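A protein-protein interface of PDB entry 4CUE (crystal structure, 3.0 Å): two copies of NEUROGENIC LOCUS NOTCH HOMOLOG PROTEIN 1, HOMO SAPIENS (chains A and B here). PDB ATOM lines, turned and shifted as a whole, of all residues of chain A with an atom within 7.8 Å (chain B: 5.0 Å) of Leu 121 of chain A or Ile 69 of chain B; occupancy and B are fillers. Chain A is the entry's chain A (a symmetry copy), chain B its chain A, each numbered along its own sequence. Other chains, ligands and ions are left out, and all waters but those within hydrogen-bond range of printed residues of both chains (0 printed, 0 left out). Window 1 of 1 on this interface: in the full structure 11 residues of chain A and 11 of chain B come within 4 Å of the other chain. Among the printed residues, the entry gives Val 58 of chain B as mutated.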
ATOM      1  N   PRO A 109      22.136  27.402  16.260  1.00  0.00           N
ATOM      2  CA  PRO A 109      22.564  25.993  16.315  1.00  0.00           C
ATOM      3  C   PRO A 109      23.333  25.673  15.036  1.00  0.00           C
ATOM      4  O   PRO A 109      23.186  26.404  14.037  1.00  0.00           O
ATOM      5  CB  PRO A 109      21.241  25.225  16.350  1.00  0.00           C
ATOM      6  CG  PRO A 109      20.264  26.098  15.667  1.00  0.00           C
ATOM      7  CD  PRO A 109      20.695  27.515  15.912  1.00  0.00           C
ATOM      8  N   THR A 110      24.131  24.592  15.042  1.00  0.00           N
ATOM      9  CA  THR A 110      24.894  24.203  13.848  1.00  0.00           C
ATOM     10  C   THR A 110      24.010  24.122  12.605  1.00  0.00           C
ATOM     11  O   THR A 110      22.897  23.596  12.648  1.00  0.00           O
ATOM     12  CB  THR A 110      25.670  22.915  14.032  1.00  0.00           C
ATOM     13  OG1 THR A 110      26.289  22.861  15.312  1.00  0.00           O
ATOM     14  CG2 THR A 110      26.763  22.786  13.015  1.00  0.00           C
ATOM     15  N   GLY A 111      24.507  24.707  11.527  1.00  0.00           N
ATOM     16  CA  GLY A 111      23.842  24.700  10.226  1.00  0.00           C
ATOM     17  C   GLY A 111      23.054  25.948   9.956  1.00  0.00           C
ATOM     18  O   GLY A 111      22.436  26.070   8.893  1.00  0.00           O
ATOM     19  N   PHE A 112      23.057  26.878  10.931  1.00  0.00           N
ATOM     20  CA  PHE A 112      22.372  28.156  10.787  1.00  0.00           C
ATOM     21  C   PHE A 112      23.291  29.337  11.092  1.00  0.00           C
ATOM     22  O   PHE A 112      24.120  29.273  12.009  1.00  0.00           O
ATOM     23  CB  PHE A 112      21.106  28.214  11.645  1.00  0.00           C
ATOM     24  CG  PHE A 112      20.029  27.252  11.221  1.00  0.00           C
ATOM     25  CD1 PHE A 112      19.160  27.572  10.193  1.00  0.00           C
ATOM     26  CD2 PHE A 112      19.902  26.003  11.838  1.00  0.00           C
ATOM     27  CE1 PHE A 112      18.171  26.664   9.795  1.00  0.00           C
ATOM     28  CE2 PHE A 112      18.917  25.098  11.438  1.00  0.00           C
ATOM     29  CZ  PHE A 112      18.045  25.444  10.439  1.00  0.00           C
ATOM     30  N   THR A 113      23.131  30.418  10.315  1.00  0.00           N
ATOM     31  CA  THR A 113      23.918  31.640  10.486  1.00  0.00           C
ATOM     32  C   THR A 113      23.075  32.898  10.232  1.00  0.00           C
ATOM     33  O   THR A 113      21.948  32.794   9.740  1.00  0.00           O
ATOM     34  CB  THR A 113      25.190  31.608   9.602  1.00  0.00           C
ATOM     35  OG1 THR A 113      26.065  32.660   9.996  1.00  0.00           O
ATOM     36  CG2 THR A 113      24.895  31.806   8.118  1.00  0.00           C
ATOM     37  N   GLY A 114      23.648  34.062  10.514  1.00  0.00           N
ATOM     38  CA  GLY A 114      22.976  35.336  10.346  1.00  0.00           C
ATOM     39  C   GLY A 114      22.591  35.905  11.687  1.00  0.00           C
ATOM     40  O   GLY A 114      22.519  35.173  12.682  1.00  0.00           O
ATOM     41  N   CYS A 117      19.707  34.108  12.803  1.00  0.00           N
ATOM     42  CA  CYS A 117      19.783  32.693  12.446  1.00  0.00           C
ATOM     43  C   CYS A 117      18.938  32.339  11.216  1.00  0.00           C
ATOM     44  O   CYS A 117      18.496  31.198  11.108  1.00  0.00           O
ATOM     45  CB  CYS A 117      19.420  31.810  13.638  1.00  0.00           C
ATOM     46  SG  CYS A 117      20.389  32.123  15.125  1.00  0.00           S
ATOM     47  N   GLN A 118      18.721  33.302  10.290  1.00  0.00           N
ATOM     48  CA  GLN A 118      17.891  33.120   9.094  1.00  0.00           C
ATOM     49  C   GLN A 118      18.440  32.108   8.121  1.00  0.00           C
ATOM     50  O   GLN A 118      17.666  31.357   7.513  1.00  0.00           O
ATOM     51  CB  GLN A 118      17.771  34.391   8.263  1.00  0.00           C
ATOM     52  CG  GLN A 118      17.331  35.658   8.932  1.00  0.00           C
ATOM     53  CD  GLN A 118      18.527  36.461   9.400  1.00  0.00           C
ATOM     54  OE1 GLN A 118      19.625  35.936   9.674  1.00  0.00           O
ATOM     55  NE2 GLN A 118      18.325  37.760   9.527  1.00  0.00           N
ATOM     56  N   VAL A 119      19.761  32.172   7.874  1.00  0.00           N
ATOM     57  CA  VAL A 119      20.400  31.379   6.841  1.00  0.00           C
ATOM     58  C   VAL A 119      20.517  29.900   7.164  1.00  0.00           C
ATOM     59  O   VAL A 119      21.195  29.537   8.122  1.00  0.00           O
ATOM     60  CB  VAL A 119      21.725  32.019   6.396  1.00  0.00           C
ATOM     61  CG1 VAL A 119      22.298  31.291   5.191  1.00  0.00           C
ATOM     62  CG2 VAL A 119      21.540  33.492   6.069  1.00  0.00           C
ATOM     63  N   ASP A 120      19.854  29.052   6.356  1.00  0.00           N
ATOM     64  CA  ASP A 120      19.968  27.610   6.502  1.00  0.00           C
ATOM     65  C   ASP A 120      21.131  27.148   5.628  1.00  0.00           C
ATOM     66  O   ASP A 120      21.191  27.483   4.446  1.00  0.00           O
ATOM     67  CB  ASP A 120      18.672  26.894   6.090  1.00  0.00           C
ATOM     68  CG  ASP A 120      18.566  25.443   6.581  1.00  0.00           C
ATOM     69  OD1 ASP A 120      19.586  24.718   6.537  1.00  0.00           O
ATOM     70  OD2 ASP A 120      17.461  25.034   7.006  1.00  0.00           O
ATOM     71  N   LEU A 121      22.047  26.382   6.205  1.00  0.00           N
ATOM     72  CA  LEU A 121      23.225  25.904   5.489  1.00  0.00           C
ATOM     73  C   LEU A 121      23.234  24.394   5.351  1.00  0.00           C
ATOM     74  O   LEU A 121      24.140  23.846   4.718  1.00  0.00           O
ATOM     75  CB  LEU A 121      24.506  26.374   6.229  1.00  0.00           C
ATOM     76  CG  LEU A 121      24.714  27.874   6.464  1.00  0.00           C
ATOM     77  CD1 LEU A 121      25.777  28.104   7.488  1.00  0.00           C
ATOM     78  CD2 LEU A 121      25.081  28.580   5.192  1.00  0.00           C
ATOM     79  N   HIS A 122      22.236  23.722   5.937  1.00  0.00           N
ATOM     80  CA  HIS A 122      22.132  22.263   5.971  1.00  0.00           C
ATOM     81  C   HIS A 122      22.053  21.618   4.601  1.00  0.00           C
ATOM     82  O   HIS A 122      22.602  20.527   4.420  1.00  0.00           O
ATOM     83  CB  HIS A 122      20.939  21.816   6.826  1.00  0.00           C
ATOM     84  CG  HIS A 122      21.121  22.021   8.295  1.00  0.00           C
ATOM     85  ND1 HIS A 122      21.836  21.117   9.064  1.00  0.00           N
ATOM     86  CD2 HIS A 122      20.648  23.004   9.100  1.00  0.00           C
ATOM     87  CE1 HIS A 122      21.773  21.572  10.307  1.00  0.00           C
ATOM     88  NE2 HIS A 122      21.067  22.707  10.378  1.00  0.00           N
ATOM     89  N   HIS A 123      21.359  22.273   3.650  1.00  0.00           N
ATOM     90  CA  HIS A 123      21.161  21.750   2.300  1.00  0.00           C
ATOM     91  C   HIS A 123      22.439  21.777   1.453  1.00  0.00           C
ATOM     92  O   HIS A 123      22.616  20.927   0.562  1.00  0.00           O
ATOM     93  CB  HIS A 123      20.030  22.502   1.600  1.00  0.00           C
ATOM     94  CG  HIS A 123      20.340  23.937   1.318  1.00  0.00           C
ATOM     95  ND1 HIS A 123      20.369  24.873   2.326  1.00  0.00           N
ATOM     96  CD2 HIS A 123      20.613  24.550   0.140  1.00  0.00           C
ATOM     97  CE1 HIS A 123      20.647  26.026   1.740  1.00  0.00           C
ATOM     98  NE2 HIS A 123      20.805  25.880   0.424  1.00  0.00           N
ATOM     99  N   ILE A 124      23.323  22.759   1.736  1.00  0.00           N
ATOM    100  CA  ILE A 124      24.596  22.928   1.037  1.00  0.00           C
ATOM    101  C   ILE A 124      25.543  21.770   1.389  1.00  0.00           C
ATOM    102  O   ILE A 124      26.287  21.298   0.518  1.00  0.00           O
ATOM    103  CB  ILE A 124      25.223  24.316   1.309  1.00  0.00           C
ATOM    104  CG1 ILE A 124      24.179  25.424   1.168  1.00  0.00           C
ATOM    105  CG2 ILE A 124      26.373  24.562   0.339  1.00  0.00           C
ATOM    106  CD1 ILE A 124      24.524  26.700   1.857  1.00  0.00           C
ATOM    107  N   LEU A 125      25.476  21.290   2.650  1.00  0.00           N
ATOM    108  CA  LEU A 125      26.288  20.175   3.143  1.00  0.00           C
ATOM    109  C   LEU A 125      25.448  18.934   3.479  1.00  0.00           C
ATOM    110  O   LEU A 125      24.892  18.294   2.584  1.00  0.00           O
ATOM    111  CB  LEU A 125      27.175  20.597   4.337  1.00  0.00           C
ATOM    112  CG  LEU A 125      26.583  21.547   5.387  1.00  0.00           C
ATOM    113  CD1 LEU A 125      25.773  20.798   6.440  1.00  0.00           C
ATOM    114  CD2 LEU A 125      27.672  22.316   6.083  1.00  0.00           C
ATOM    115  N   ALA B  57      33.946  29.994  10.095  1.00  0.00           N
ATOM    116  CA  ALA B  57      33.346  29.860   8.783  1.00  0.00           C
ATOM    117  C   ALA B  57      33.111  28.387   8.486  1.00  0.00           C
ATOM    118  O   ALA B  57      33.744  27.512   9.095  1.00  0.00           O
ATOM    119  CB  ALA B  57      34.253  30.475   7.734  1.00  0.00           C
ATOM    120  N   VAL B  58      32.163  28.127   7.573  1.00  0.00           N
ATOM    121  CA  VAL B  58      31.806  26.789   7.101  1.00  0.00           C
ATOM    122  C   VAL B  58      32.676  26.502   5.876  1.00  0.00           C
ATOM    123  O   VAL B  58      32.689  27.306   4.932  1.00  0.00           O
ATOM    124  CB  VAL B  58      30.288  26.725   6.760  1.00  0.00           C
ATOM    125  CG1 VAL B  58      29.909  25.457   6.003  1.00  0.00           C
ATOM    126  CG2 VAL B  58      29.439  26.875   8.007  1.00  0.00           C
ATOM    127  N   LEU B  60      33.392  24.361   2.502  1.00  0.00           N
ATOM    128  CA  LEU B  60      32.791  23.514   1.466  1.00  0.00           C
ATOM    129  C   LEU B  60      33.898  22.838   0.679  1.00  0.00           C
ATOM    130  O   LEU B  60      34.717  23.505   0.044  1.00  0.00           O
ATOM    131  CB  LEU B  60      31.899  24.301   0.503  1.00  0.00           C
ATOM    132  CG  LEU B  60      30.792  25.133   1.105  1.00  0.00           C
ATOM    133  CD1 LEU B  60      30.085  25.912   0.017  1.00  0.00           C
ATOM    134  CD2 LEU B  60      29.827  24.281   1.948  1.00  0.00           C
ATOM    135  N   GLN B  67      35.528  26.405  -0.590  1.00  0.00           N
ATOM    136  CA  GLN B  67      34.881  27.696  -0.499  1.00  0.00           C
ATOM    137  C   GLN B  67      34.496  27.836   0.943  1.00  0.00           C
ATOM    138  O   GLN B  67      34.143  26.850   1.616  1.00  0.00           O
ATOM    139  CB  GLN B  67      33.662  27.849  -1.411  1.00  0.00           C
ATOM    140  CG  GLN B  67      34.026  28.190  -2.842  1.00  0.00           C
ATOM    141  CD  GLN B  67      32.839  28.596  -3.691  1.00  0.00           C
ATOM    142  OE1 GLN B  67      31.800  27.921  -3.741  1.00  0.00           O
ATOM    143  NE2 GLN B  67      32.983  29.693  -4.428  1.00  0.00           N
ATOM    144  N   CYS B  68      34.650  29.050   1.448  1.00  0.00           N
ATOM    145  CA  CYS B  68      34.318  29.339   2.817  1.00  0.00           C
ATOM    146  C   CYS B  68      33.003  30.099   2.815  1.00  0.00           C
ATOM    147  O   CYS B  68      32.732  30.940   1.933  1.00  0.00           O
ATOM    148  CB  CYS B  68      35.429  30.144   3.496  1.00  0.00           C
ATOM    149  SG  CYS B  68      37.051  29.322   3.573  1.00  0.00           S
ATOM    150  N   ILE B  69      32.162  29.780   3.789  1.00  0.00           N
ATOM    151  CA  ILE B  69      30.932  30.530   4.010  1.00  0.00           C
ATOM    152  C   ILE B  69      31.242  31.282   5.276  1.00  0.00           C
ATOM    153  O   ILE B  69      31.505  30.662   6.306  1.00  0.00           O
ATOM    154  CB  ILE B  69      29.661  29.658   4.127  1.00  0.00           C
ATOM    155  CG1 ILE B  69      29.529  28.716   2.932  1.00  0.00           C
ATOM    156  CG2 ILE B  69      28.409  30.558   4.265  1.00  0.00           C
ATOM    157  CD1 ILE B  69      28.471  27.657   3.119  1.00  0.00           C
ATOM    158  N   CYS B  70      31.283  32.607   5.176  1.00  0.00           N
ATOM    159  CA  CYS B  70      31.669  33.458   6.280  1.00  0.00           C
ATOM    160  C   CYS B  70      30.531  33.712   7.230  1.00  0.00           C
ATOM    161  O   CYS B  70      29.367  33.761   6.825  1.00  0.00           O
ATOM    162  CB  CYS B  70      32.262  34.775   5.773  1.00  0.00           C
ATOM    163  SG  CYS B  70      33.676  34.604   4.631  1.00  0.00           S
ATOM    164  N   MET B  71      30.889  33.899   8.501  1.00  0.00           N
ATOM    165  CA  MET B  71      29.978  34.356   9.540  1.00  0.00           C
ATOM    166  C   MET B  71      29.737  35.854   9.249  1.00  0.00           C
ATOM    167  O   MET B  71      30.567  36.504   8.599  1.00  0.00           O
ATOM    168  CB  MET B  71      30.587  34.137  10.951  1.00  0.00           C
ATOM    169  CG  MET B  71      30.771  32.658  11.334  1.00  0.00           C
ATOM    170  SD  MET B  71      29.677  31.460  10.442  1.00  0.00           S
ATOM    171  CE  MET B  71      28.280  31.512  11.582  1.00  0.00           C
ATOM    172  N   CYS B  79      37.796  33.946   4.970  1.00  0.00           N
ATOM    173  CA  CYS B  79      36.953  34.666   5.936  1.00  0.00           C
ATOM    174  C   CYS B  79      37.841  35.330   6.982  1.00  0.00           C
ATOM    175  O   CYS B  79      37.464  35.491   8.137  1.00  0.00           O
ATOM    176  CB  CYS B  79      35.926  33.735   6.569  1.00  0.00           C
ATOM    177  SG  CYS B  79      34.765  33.034   5.375  1.00  0.00           S
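The backbone NH of Ile 69 of chain B is in hydrogen-bond range of the backbone carbonyl oxygen of Val 58 of chain B, at 2.8 Å.
N of Gln 118 of chain A sits at hydrogen-bond distance from O of Thr 113 of chain A (3.3 Å).
The backbone NH of Leu 60 of chain B sits at hydrogen-bond distance from the backbone carbonyl oxygen of Gln 67 of chain B, at 2.7 Å.
The backbone NH of Leu 121 of chain A lies within hydrogen-bond range of the backbone carbonyl oxygen of Gly 111 of chain A, 2.7 Å away.
N of Val 119 of chain A is in hydrogen-bond range of O of Thr 113 of chain A (2.9 Å).
SG of Cys 70 of chain B forms a disulfide with SG of Cys 79 of chain B (2.1 Å).
Among the printed residues, pairs that only touch across the chains: Thr 113 of chain A with Met 71 of chain B (3.0 Å), Ile 124 of chain A with Leu 60 of chain B (3.8 Å), Leu 125 of chain A with Val 58 of chain B (3.9 Å), Leu 121 of chain A with Val 58 of chain B (3.9 Å) and Leu 121 of chain A with Ile 69 of chain B (3.98 Å).
Printed residues of chain B within 4 Å of Leu 121 of chain A: Val 58 (3.9 Å) and Ile 69 (3.98 Å).
Printed residues of chain A within 4 Å of Ile 69 of chain B: Leu 121 (3.98 Å).
Of the printed residues of chain A, Val 58 of chain B touches Leu 121 and Leu 125.
Of the printed residues of chain B, Thr 113 of chain A touches Met 71 (3.0 Å).
Of the printed residues of chain B, Leu 125 of chain A touches Val 58.
Printed residues of chain A within 4 Å of Leu 60 of chain B: Ile 124.
The nearest printed residue of chain A that does not touch Leu 60 of chain B is Leu 125 of chain A (5.1 Å).
Printed residues of chain B that touch a printed residue of chain A: Val 58, Leu 60, Ile 69 and Met 71.
Hydrophobic or aromatic side chains of chain B that line the printed part of chain A: Val 58, Leu 60, Ile 69 and Met 71.
Printed residues of chain A that touch a printed residue of chain B: Thr 113, Leu 121, Ile 124 and Leu 125.
Hydrophobic or aromatic side chains of chain A that line the printed part of chain B: Leu 121, Ile 124 and Leu 125.
Along chain A the printed residues that touch a printed residue of chain B span positions 113 to 125.
Among the printed residues, 5 pairs touch across the chains.
Among the printed residues, no Asp or Glu carboxylate lies within 4 Å of a Lys or Arg side-chain nitrogen of the other chain.
No position is printed for both chains.
Of the 5 pairs that touch across the chains among the printed residues, none has its exchanged pair printed and touching as well.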
